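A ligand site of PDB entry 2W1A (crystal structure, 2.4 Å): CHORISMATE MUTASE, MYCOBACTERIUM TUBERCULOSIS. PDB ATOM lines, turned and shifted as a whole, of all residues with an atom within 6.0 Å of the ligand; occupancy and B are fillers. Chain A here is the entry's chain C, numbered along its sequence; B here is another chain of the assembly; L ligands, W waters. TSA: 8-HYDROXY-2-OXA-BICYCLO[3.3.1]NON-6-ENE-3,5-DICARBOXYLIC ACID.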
ATOM      1  N   ARG A  35      -5.892 -11.791 -10.691  1.00  0.00           N
ATOM      2  CA  ARG A  35      -5.415 -10.644 -11.488  1.00  0.00           C
ATOM      3  C   ARG A  35      -3.932 -10.738 -11.821  1.00  0.00           C
ATOM      4  O   ARG A  35      -3.528 -10.446 -12.952  1.00  0.00           O
ATOM      5  CB  ARG A  35      -5.667  -9.340 -10.733  1.00  0.00           C
ATOM      6  CG  ARG A  35      -5.710  -8.120 -11.619  1.00  0.00           C
ATOM      7  CD  ARG A  35      -5.668  -6.837 -10.808  1.00  0.00           C
ATOM      8  NE  ARG A  35      -5.609  -5.663 -11.681  1.00  0.00           N
ATOM      9  CZ  ARG A  35      -4.503  -5.239 -12.281  1.00  0.00           C
ATOM     10  NH1 ARG A  35      -3.341  -5.885 -12.159  1.00  0.00           N
ATOM     11  NH2 ARG A  35      -4.570  -4.156 -13.043  1.00  0.00           N
ATOM     12  N   VAL A  38      -3.381 -13.236 -14.630  1.00  0.00           N
ATOM     13  CA  VAL A  38      -3.853 -12.698 -15.915  1.00  0.00           C
ATOM     14  C   VAL A  38      -2.864 -11.667 -16.473  1.00  0.00           C
ATOM     15  O   VAL A  38      -2.538 -11.691 -17.655  1.00  0.00           O
ATOM     16  CB  VAL A  38      -5.263 -12.061 -15.764  1.00  0.00           C
ATOM     17  CG1 VAL A  38      -5.705 -11.405 -17.067  1.00  0.00           C
ATOM     18  CG2 VAL A  38      -6.274 -13.110 -15.343  1.00  0.00           C
ATOM     19  N   SER A  39      -2.401 -10.780 -15.597  1.00  0.00           N
ATOM     20  CA  SER A  39      -1.383  -9.783 -15.929  1.00  0.00           C
ATOM     21  C   SER A  39      -0.094 -10.431 -16.447  1.00  0.00           C
ATOM     22  O   SER A  39       0.448 -10.039 -17.492  1.00  0.00           O
ATOM     23  CB  SER A  39      -1.073  -8.942 -14.687  1.00  0.00           C
ATOM     24  OG  SER A  39      -0.106  -7.938 -14.952  1.00  0.00           O
ATOM     25  N   ILE A  42      -0.578 -11.797 -19.964  1.00  0.00           N
ATOM     26  CA  ILE A  42      -0.604 -10.743 -20.988  1.00  0.00           C
ATOM     27  C   ILE A  42       0.824 -10.307 -21.332  1.00  0.00           C
ATOM     28  O   ILE A  42       1.167 -10.151 -22.511  1.00  0.00           O
ATOM     29  CB  ILE A  42      -1.398  -9.507 -20.519  1.00  0.00           C
ATOM     30  CG1 ILE A  42      -2.874  -9.842 -20.314  1.00  0.00           C
ATOM     31  CG2 ILE A  42      -1.252  -8.372 -21.531  1.00  0.00           C
ATOM     32  CD1 ILE A  42      -3.627  -8.842 -19.448  1.00  0.00           C
ATOM     33  N   GLY A  43       1.640 -10.098 -20.300  1.00  0.00           N
ATOM     34  CA  GLY A  43       3.041  -9.716 -20.471  1.00  0.00           C
ATOM     35  C   GLY A  43       3.875 -10.792 -21.138  1.00  0.00           C
ATOM     36  O   GLY A  43       4.785 -10.486 -21.906  1.00  0.00           O
ATOM     37  N   ARG A  46       2.776 -10.766 -24.913  1.00  0.00           N
ATOM     38  CA  ARG A  46       3.312  -9.590 -25.617  1.00  0.00           C
ATOM     39  C   ARG A  46       4.814  -9.672 -25.808  1.00  0.00           C
ATOM     40  O   ARG A  46       5.308  -9.378 -26.900  1.00  0.00           O
ATOM     41  CB  ARG A  46       2.983  -8.291 -24.867  1.00  0.00           C
ATOM     42  CG  ARG A  46       3.637  -7.057 -25.493  1.00  0.00           C
ATOM     43  CD  ARG A  46       3.086  -5.738 -24.954  1.00  0.00           C
ATOM     44  NE  ARG A  46       3.175  -5.647 -23.500  1.00  0.00           N
ATOM     45  CZ  ARG A  46       2.162  -5.828 -22.653  1.00  0.00           C
ATOM     46  NH1 ARG A  46       0.937  -6.104 -23.094  1.00  0.00           N
ATOM     47  NH2 ARG A  46       2.369  -5.725 -21.362  1.00  0.00           N
ATOM     48  N   ARG A  53       7.926  -4.961 -22.096  1.00  0.00           N
ATOM     49  CA  ARG A  53       7.575  -5.594 -20.814  1.00  0.00           C
ATOM     50  C   ARG A  53       6.350  -4.922 -20.207  1.00  0.00           C
ATOM     51  O   ARG A  53       5.375  -5.573 -19.828  1.00  0.00           O
ATOM     52  CB  ARG A  53       8.784  -5.494 -19.860  1.00  0.00           C
ATOM     53  CG  ARG A  53       8.938  -6.636 -18.865  1.00  0.00           C
ATOM     54  CD  ARG A  53       8.525  -6.284 -17.457  1.00  0.00           C
ATOM     55  NE  ARG A  53       9.502  -6.779 -16.477  1.00  0.00           N
ATOM     56  CZ  ARG A  53       9.693  -8.058 -16.169  1.00  0.00           C
ATOM     57  NH1 ARG A  53      10.615  -8.376 -15.244  1.00  0.00           N
ATOM     58  NH2 ARG A  53       8.995  -9.037 -16.754  1.00  0.00           N
ATOM     59  N   LEU A  54       6.425  -3.585 -20.140  1.00  0.00           N
ATOM     60  CA  LEU A  54       5.407  -2.732 -19.553  1.00  0.00           C
ATOM     61  C   LEU A  54       4.837  -1.830 -20.644  1.00  0.00           C
ATOM     62  O   LEU A  54       5.491  -1.573 -21.651  1.00  0.00           O
ATOM     63  CB  LEU A  54       6.035  -1.864 -18.452  1.00  0.00           C
ATOM     64  CG  LEU A  54       6.954  -2.555 -17.455  1.00  0.00           C
ATOM     65  CD1 LEU A  54       7.619  -1.513 -16.554  1.00  0.00           C
ATOM     66  CD2 LEU A  54       6.216  -3.598 -16.630  1.00  0.00           C
ATOM     67  N   VAL A  55       3.612  -1.339 -20.424  1.00  0.00           N
ATOM     68  CA  VAL A  55       2.957  -0.413 -21.342  1.00  0.00           C
ATOM     69  C   VAL A  55       2.446   0.794 -20.544  1.00  0.00           C
ATOM     70  O   VAL A  55       1.449   0.705 -19.825  1.00  0.00           O
ATOM     71  CB  VAL A  55       1.800  -1.094 -22.111  1.00  0.00           C
ATOM     72  CG1 VAL A  55       1.188  -0.120 -23.109  1.00  0.00           C
ATOM     73  CG2 VAL A  55       2.303  -2.335 -22.827  1.00  0.00           C
ATOM     74  N   HIS A  56       3.135   1.912 -20.689  1.00  0.00           N
ATOM     75  CA  HIS A  56       2.950   3.081 -19.832  1.00  0.00           C
ATOM     76  C   HIS A  56       1.514   3.605 -19.776  1.00  0.00           C
ATOM     77  O   HIS A  56       0.984   3.840 -18.685  1.00  0.00           O
ATOM     78  CB  HIS A  56       3.893   4.201 -20.283  1.00  0.00           C
ATOM     79  CG  HIS A  56       4.043   5.288 -19.269  1.00  0.00           C
ATOM     80  ND1 HIS A  56       4.701   5.090 -18.075  1.00  0.00           N
ATOM     81  CD2 HIS A  56       3.643   6.578 -19.278  1.00  0.00           C
ATOM     82  CE1 HIS A  56       4.693   6.222 -17.379  1.00  0.00           C
ATOM     83  NE2 HIS A  56       4.060   7.145 -18.091  1.00  0.00           N
ATOM     84  N   ARG A  58      -1.277   2.157 -20.489  1.00  0.00           N
ATOM     85  CA  ARG A  58      -2.183   1.182 -19.906  1.00  0.00           C
ATOM     86  C   ARG A  58      -2.135   1.234 -18.362  1.00  0.00           C
ATOM     87  O   ARG A  58      -3.168   1.253 -17.693  1.00  0.00           O
ATOM     88  CB  ARG A  58      -1.864  -0.224 -20.404  1.00  0.00           C
ATOM     89  CG  ARG A  58      -2.754  -1.328 -19.817  1.00  0.00           C
ATOM     90  CD  ARG A  58      -4.242  -1.043 -19.979  1.00  0.00           C
ATOM     91  NE  ARG A  58      -5.057  -2.184 -19.552  1.00  0.00           N
ATOM     92  CZ  ARG A  58      -6.339  -2.357 -19.849  1.00  0.00           C
ATOM     93  NH1 ARG A  58      -6.988  -1.482 -20.601  1.00  0.00           N
ATOM     94  NH2 ARG A  58      -6.974  -3.439 -19.411  1.00  0.00           N
ATOM     95  N   GLU A  59      -0.923   1.261 -17.809  1.00  0.00           N
ATOM     96  CA  GLU A  59      -0.739   1.403 -16.356  1.00  0.00           C
ATOM     97  C   GLU A  59      -1.358   2.705 -15.813  1.00  0.00           C
ATOM     98  O   GLU A  59      -1.807   2.745 -14.671  1.00  0.00           O
ATOM     99  CB  GLU A  59       0.746   1.311 -15.977  1.00  0.00           C
ATOM    100  CG  GLU A  59       1.324  -0.084 -16.211  1.00  0.00           C
ATOM    101  CD  GLU A  59       2.633  -0.361 -15.477  1.00  0.00           C
ATOM    102  OE1 GLU A  59       3.120   0.496 -14.723  1.00  0.00           O
ATOM    103  OE2 GLU A  59       3.175  -1.469 -15.678  1.00  0.00           O
ATOM    104  N   VAL A  62      -5.067   1.971 -15.445  1.00  0.00           N
ATOM    105  CA  VAL A  62      -5.241   1.127 -14.255  1.00  0.00           C
ATOM    106  C   VAL A  62      -5.165   1.962 -12.972  1.00  0.00           C
ATOM    107  O   VAL A  62      -5.936   1.734 -12.048  1.00  0.00           O
ATOM    108  CB  VAL A  62      -4.206  -0.031 -14.238  1.00  0.00           C
ATOM    109  CG1 VAL A  62      -4.304  -0.834 -12.950  1.00  0.00           C
ATOM    110  CG2 VAL A  62      -4.404  -0.929 -15.457  1.00  0.00           C
ATOM    111  N   ARG A  65      -8.634   4.227 -12.660  1.00  0.00           N
ATOM    112  CA  ARG A  65      -9.882   3.585 -12.248  1.00  0.00           C
ATOM    113  C   ARG A  65      -9.932   3.112 -10.790  1.00  0.00           C
ATOM    114  O   ARG A  65     -10.862   2.397 -10.403  1.00  0.00           O
ATOM    115  CB  ARG A  65     -10.269   2.451 -13.201  1.00  0.00           C
ATOM    116  CG  ARG A  65      -9.355   1.228 -13.226  1.00  0.00           C
ATOM    117  CD  ARG A  65      -9.550   0.579 -14.576  1.00  0.00           C
ATOM    118  NE  ARG A  65      -8.791  -0.645 -14.798  1.00  0.00           N
ATOM    119  CZ  ARG A  65      -8.704  -1.256 -15.980  1.00  0.00           C
ATOM    120  NH1 ARG A  65      -9.321  -0.753 -17.049  1.00  0.00           N
ATOM    121  NH2 ARG A  65      -7.990  -2.372 -16.105  1.00  0.00           N
ATOM    122  N   LEU A  80      -1.052  -3.408  -7.280  1.00  0.00           N
ATOM    123  CA  LEU A  80      -1.577  -4.464  -8.144  1.00  0.00           C
ATOM    124  C   LEU A  80      -0.754  -4.622  -9.431  1.00  0.00           C
ATOM    125  O   LEU A  80      -0.621  -5.726  -9.952  1.00  0.00           O
ATOM    126  CB  LEU A  80      -3.047  -4.223  -8.491  1.00  0.00           C
ATOM    127  CG  LEU A  80      -4.078  -4.314  -7.355  1.00  0.00           C
ATOM    128  CD1 LEU A  80      -5.482  -4.076  -7.894  1.00  0.00           C
ATOM    129  CD2 LEU A  80      -3.988  -5.645  -6.643  1.00  0.00           C
ATOM    130  N   LEU A  81      -0.217  -3.523  -9.953  1.00  0.00           N
ATOM    131  CA  LEU A  81       0.695  -3.599 -11.094  1.00  0.00           C
ATOM    132  C   LEU A  81       1.976  -4.342 -10.697  1.00  0.00           C
ATOM    133  O   LEU A  81       2.466  -5.169 -11.453  1.00  0.00           O
ATOM    134  CB  LEU A  81       1.022  -2.192 -11.631  1.00  0.00           C
ATOM    135  CG  LEU A  81      -0.152  -1.424 -12.260  1.00  0.00           C
ATOM    136  CD1 LEU A  81       0.175   0.062 -12.432  1.00  0.00           C
ATOM    137  CD2 LEU A  81      -0.569  -2.026 -13.571  1.00  0.00           C
ATOM    138  N   GLY A  84       1.473  -8.008 -10.688  1.00  0.00           N
ATOM    139  CA  GLY A  84       1.299  -8.538 -12.046  1.00  0.00           C
ATOM    140  C   GLY A  84       2.560  -8.568 -12.897  1.00  0.00           C
ATOM    141  O   GLY A  84       2.945  -9.632 -13.387  1.00  0.00           O
ATOM    142  N   ARG A  85       3.188  -7.411 -13.083  1.00  0.00           N
ATOM    143  CA  ARG A  85       4.404  -7.320 -13.917  1.00  0.00           C
ATOM    144  C   ARG A  85       5.723  -7.254 -13.130  1.00  0.00           C
ATOM    145  O   ARG A  85       6.805  -7.222 -13.735  1.00  0.00           O
ATOM    146  CB  ARG A  85       4.315  -6.157 -14.930  1.00  0.00           C
ATOM    147  CG  ARG A  85       3.820  -4.805 -14.419  1.00  0.00           C
ATOM    148  CD  ARG A  85       4.809  -4.108 -13.490  1.00  0.00           C
ATOM    149  NE  ARG A  85       4.465  -2.697 -13.317  1.00  0.00           N
ATOM    150  CZ  ARG A  85       4.823  -1.937 -12.278  1.00  0.00           C
ATOM    151  NH1 ARG A  85       5.526  -2.434 -11.275  1.00  0.00           N
ATOM    152  NH2 ARG A  85       4.446  -0.663 -12.245  1.00  0.00           N
ATOM    153  N   ILE B  14      -4.691 -10.681 -26.116  1.00  0.00           N
ATOM    154  CA  ILE B  14      -4.425  -9.589 -25.168  1.00  0.00           C
ATOM    155  C   ILE B  14      -5.681  -8.750 -24.943  1.00  0.00           C
ATOM    156  O   ILE B  14      -5.973  -8.347 -23.824  1.00  0.00           O
ATOM    157  CB  ILE B  14      -3.259  -8.683 -25.656  1.00  0.00           C
ATOM    158  CG1 ILE B  14      -1.958  -9.475 -25.764  1.00  0.00           C
ATOM    159  CG2 ILE B  14      -3.054  -7.496 -24.694  1.00  0.00           C
ATOM    160  CD1 ILE B  14      -0.838  -8.725 -26.461  1.00  0.00           C
ATOM    161  N   ARG B  18      -7.258  -8.532 -21.293  1.00  0.00           N
ATOM    162  CA  ARG B  18      -7.459  -7.202 -20.726  1.00  0.00           C
ATOM    163  C   ARG B  18      -8.924  -6.952 -20.365  1.00  0.00           C
ATOM    164  O   ARG B  18      -9.210  -6.214 -19.429  1.00  0.00           O
ATOM    165  CB  ARG B  18      -6.964  -6.110 -21.687  1.00  0.00           C
ATOM    166  CG  ARG B  18      -5.458  -5.876 -21.641  1.00  0.00           C
ATOM    167  CD  ARG B  18      -5.075  -4.660 -22.454  1.00  0.00           C
ATOM    168  NE  ARG B  18      -3.626  -4.446 -22.490  1.00  0.00           N
ATOM    169  CZ  ARG B  18      -3.039  -3.453 -23.162  1.00  0.00           C
ATOM    170  NH1 ARG B  18      -3.761  -2.588 -23.877  1.00  0.00           N
ATOM    171  NH2 ARG B  18      -1.721  -3.325 -23.130  1.00  0.00           N
ATOM    172  N   ILE B  21      -9.222  -8.407 -16.822  1.00  0.00           N
ATOM    173  CA  ILE B  21      -8.568  -7.496 -15.873  1.00  0.00           C
ATOM    174  C   ILE B  21      -9.536  -6.361 -15.542  1.00  0.00           C
ATOM    175  O   ILE B  21      -9.677  -5.996 -14.374  1.00  0.00           O
ATOM    176  CB  ILE B  21      -7.192  -6.953 -16.401  1.00  0.00           C
ATOM    177  CG1 ILE B  21      -6.039  -7.840 -15.930  1.00  0.00           C
ATOM    178  CG2 ILE B  21      -6.926  -5.521 -15.905  1.00  0.00           C
ATOM    179  CD1 ILE B  21      -4.722  -7.505 -16.558  1.00  0.00           C
ATOM    180  N   ASP B  25     -10.881  -5.548 -11.888  1.00  0.00           N
ATOM    181  CA  ASP B  25     -10.608  -4.257 -11.239  1.00  0.00           C
ATOM    182  C   ASP B  25     -11.878  -3.542 -10.736  1.00  0.00           C
ATOM    183  O   ASP B  25     -11.815  -2.794  -9.771  1.00  0.00           O
ATOM    184  CB  ASP B  25      -9.820  -3.307 -12.157  1.00  0.00           C
ATOM    185  CG  ASP B  25      -8.325  -3.603 -12.182  1.00  0.00           C
ATOM    186  OD1 ASP B  25      -7.754  -4.018 -11.144  1.00  0.00           O
ATOM    187  OD2 ASP B  25      -7.698  -3.413 -13.240  1.00  0.00           O
HETATM  188  C1  TSA L   1      -0.728  -4.743 -16.638  1.00  0.00           C
HETATM  189  C2  TSA L   1      -0.936  -3.357 -17.213  1.00  0.00           C
HETATM  190  C3  TSA L   1      -0.042  -2.768 -18.015  1.00  0.00           C
HETATM  191  C4  TSA L   1       1.265  -3.437 -18.437  1.00  0.00           C
HETATM  192  O5  TSA L   1       2.379  -2.617 -18.042  1.00  0.00           O
HETATM  193  C5  TSA L   1       1.414  -4.852 -17.848  1.00  0.00           C
HETATM  194  C6  TSA L   1       0.770  -4.953 -16.471  1.00  0.00           C
HETATM  195  O7  TSA L   1       0.870  -5.852 -18.744  1.00  0.00           O
HETATM  196  C8  TSA L   1      -0.561  -6.011 -18.871  1.00  0.00           C
HETATM  197  C9  TSA L   1      -1.289  -5.856 -17.533  1.00  0.00           C
HETATM  198  C10 TSA L   1      -1.483  -4.900 -15.333  1.00  0.00           C
HETATM  199  O1  TSA L   1      -2.628  -4.407 -15.262  1.00  0.00           O
HETATM  200  O2  TSA L   1      -0.961  -5.533 -14.385  1.00  0.00           O
HETATM  201  C11 TSA L   1      -1.214  -5.109 -19.903  1.00  0.00           C
HETATM  202  O3  TSA L   1      -0.498  -4.527 -20.738  1.00  0.00           O
HETATM  203  O4  TSA L   1      -2.450  -4.938 -19.897  1.00  0.00           O
HETATM  204  O   HOH W   1      -4.361  -4.447 -17.440  1.00  0.00           O
HETATM  205  O   HOH W   2       2.361  -7.960 -17.508  1.00  0.00           O
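The side-chain hydroxyl (OG) of Ser 39 sits at hydrogen-bond distance from an oxygen (O2) of the ligand, at 2.6 Å. The side-chain carboxylate (OE2) of Glu 59 lies within hydrogen-bond range of an oxygen (O5) of the ligand (2.7 Å). NE of Arg 18 of chain B is in salt-bridge range of O4 of the ligand (2.9 Å). The guanidinium group of Arg 35 is in salt-bridge range of an oxygen (O1) of the ligand, 3.0 Å away. The backbone NH (N) of Val 55 is in hydrogen-bond range of an oxygen (O5) of the ligand, 3.0 Å away. The guanidinium group of Arg 46 lies within salt-bridge range of an oxygen (O3) of the ligand, at 3.2 Å. The guanidinium group (NE) of Arg 58 lies within salt-bridge range of an oxygen (O4) of the ligand (3.8 Å).
The side-chain carboxylate (OE2) of Glu 59 is in salt-bridge range of the guanidinium group (NE) of Arg 85, at 3.0 Å. The guanidinium group of Arg 35 lies within salt-bridge range of the side-chain carboxylate of Asp 25 of chain B. The guanidinium group (NH2) of Arg 46 lies within hydrogen-bond range of the backbone carbonyl oxygen (O) of Arg 53, at 3.4 Å.
Residues that only touch the ligand: Leu 54, Leu 81, Ile 42, Arg 85, Val 62 and Ile 21 of chain B. Within 4 Å of the ligand: Arg 35, Ser 39, Ile 42, Arg 46, Leu 54, Val 55, Arg 58, Glu 59, Val 62, Leu 81, Arg 85, Arg 18 of chain B and Ile 21 of chain B. The nearest printed residue that does not touch the ligand is Gly 84 (4.4 Å).
Water W1 lies within hydrogen-bond range of O1 of the ligand (2.8 Å) and NE of Arg 58 (3.2 Å). Water W2 bridges the backbone carbonyl oxygen (O) of Ser 39 and an oxygen (O7) of the ligand.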
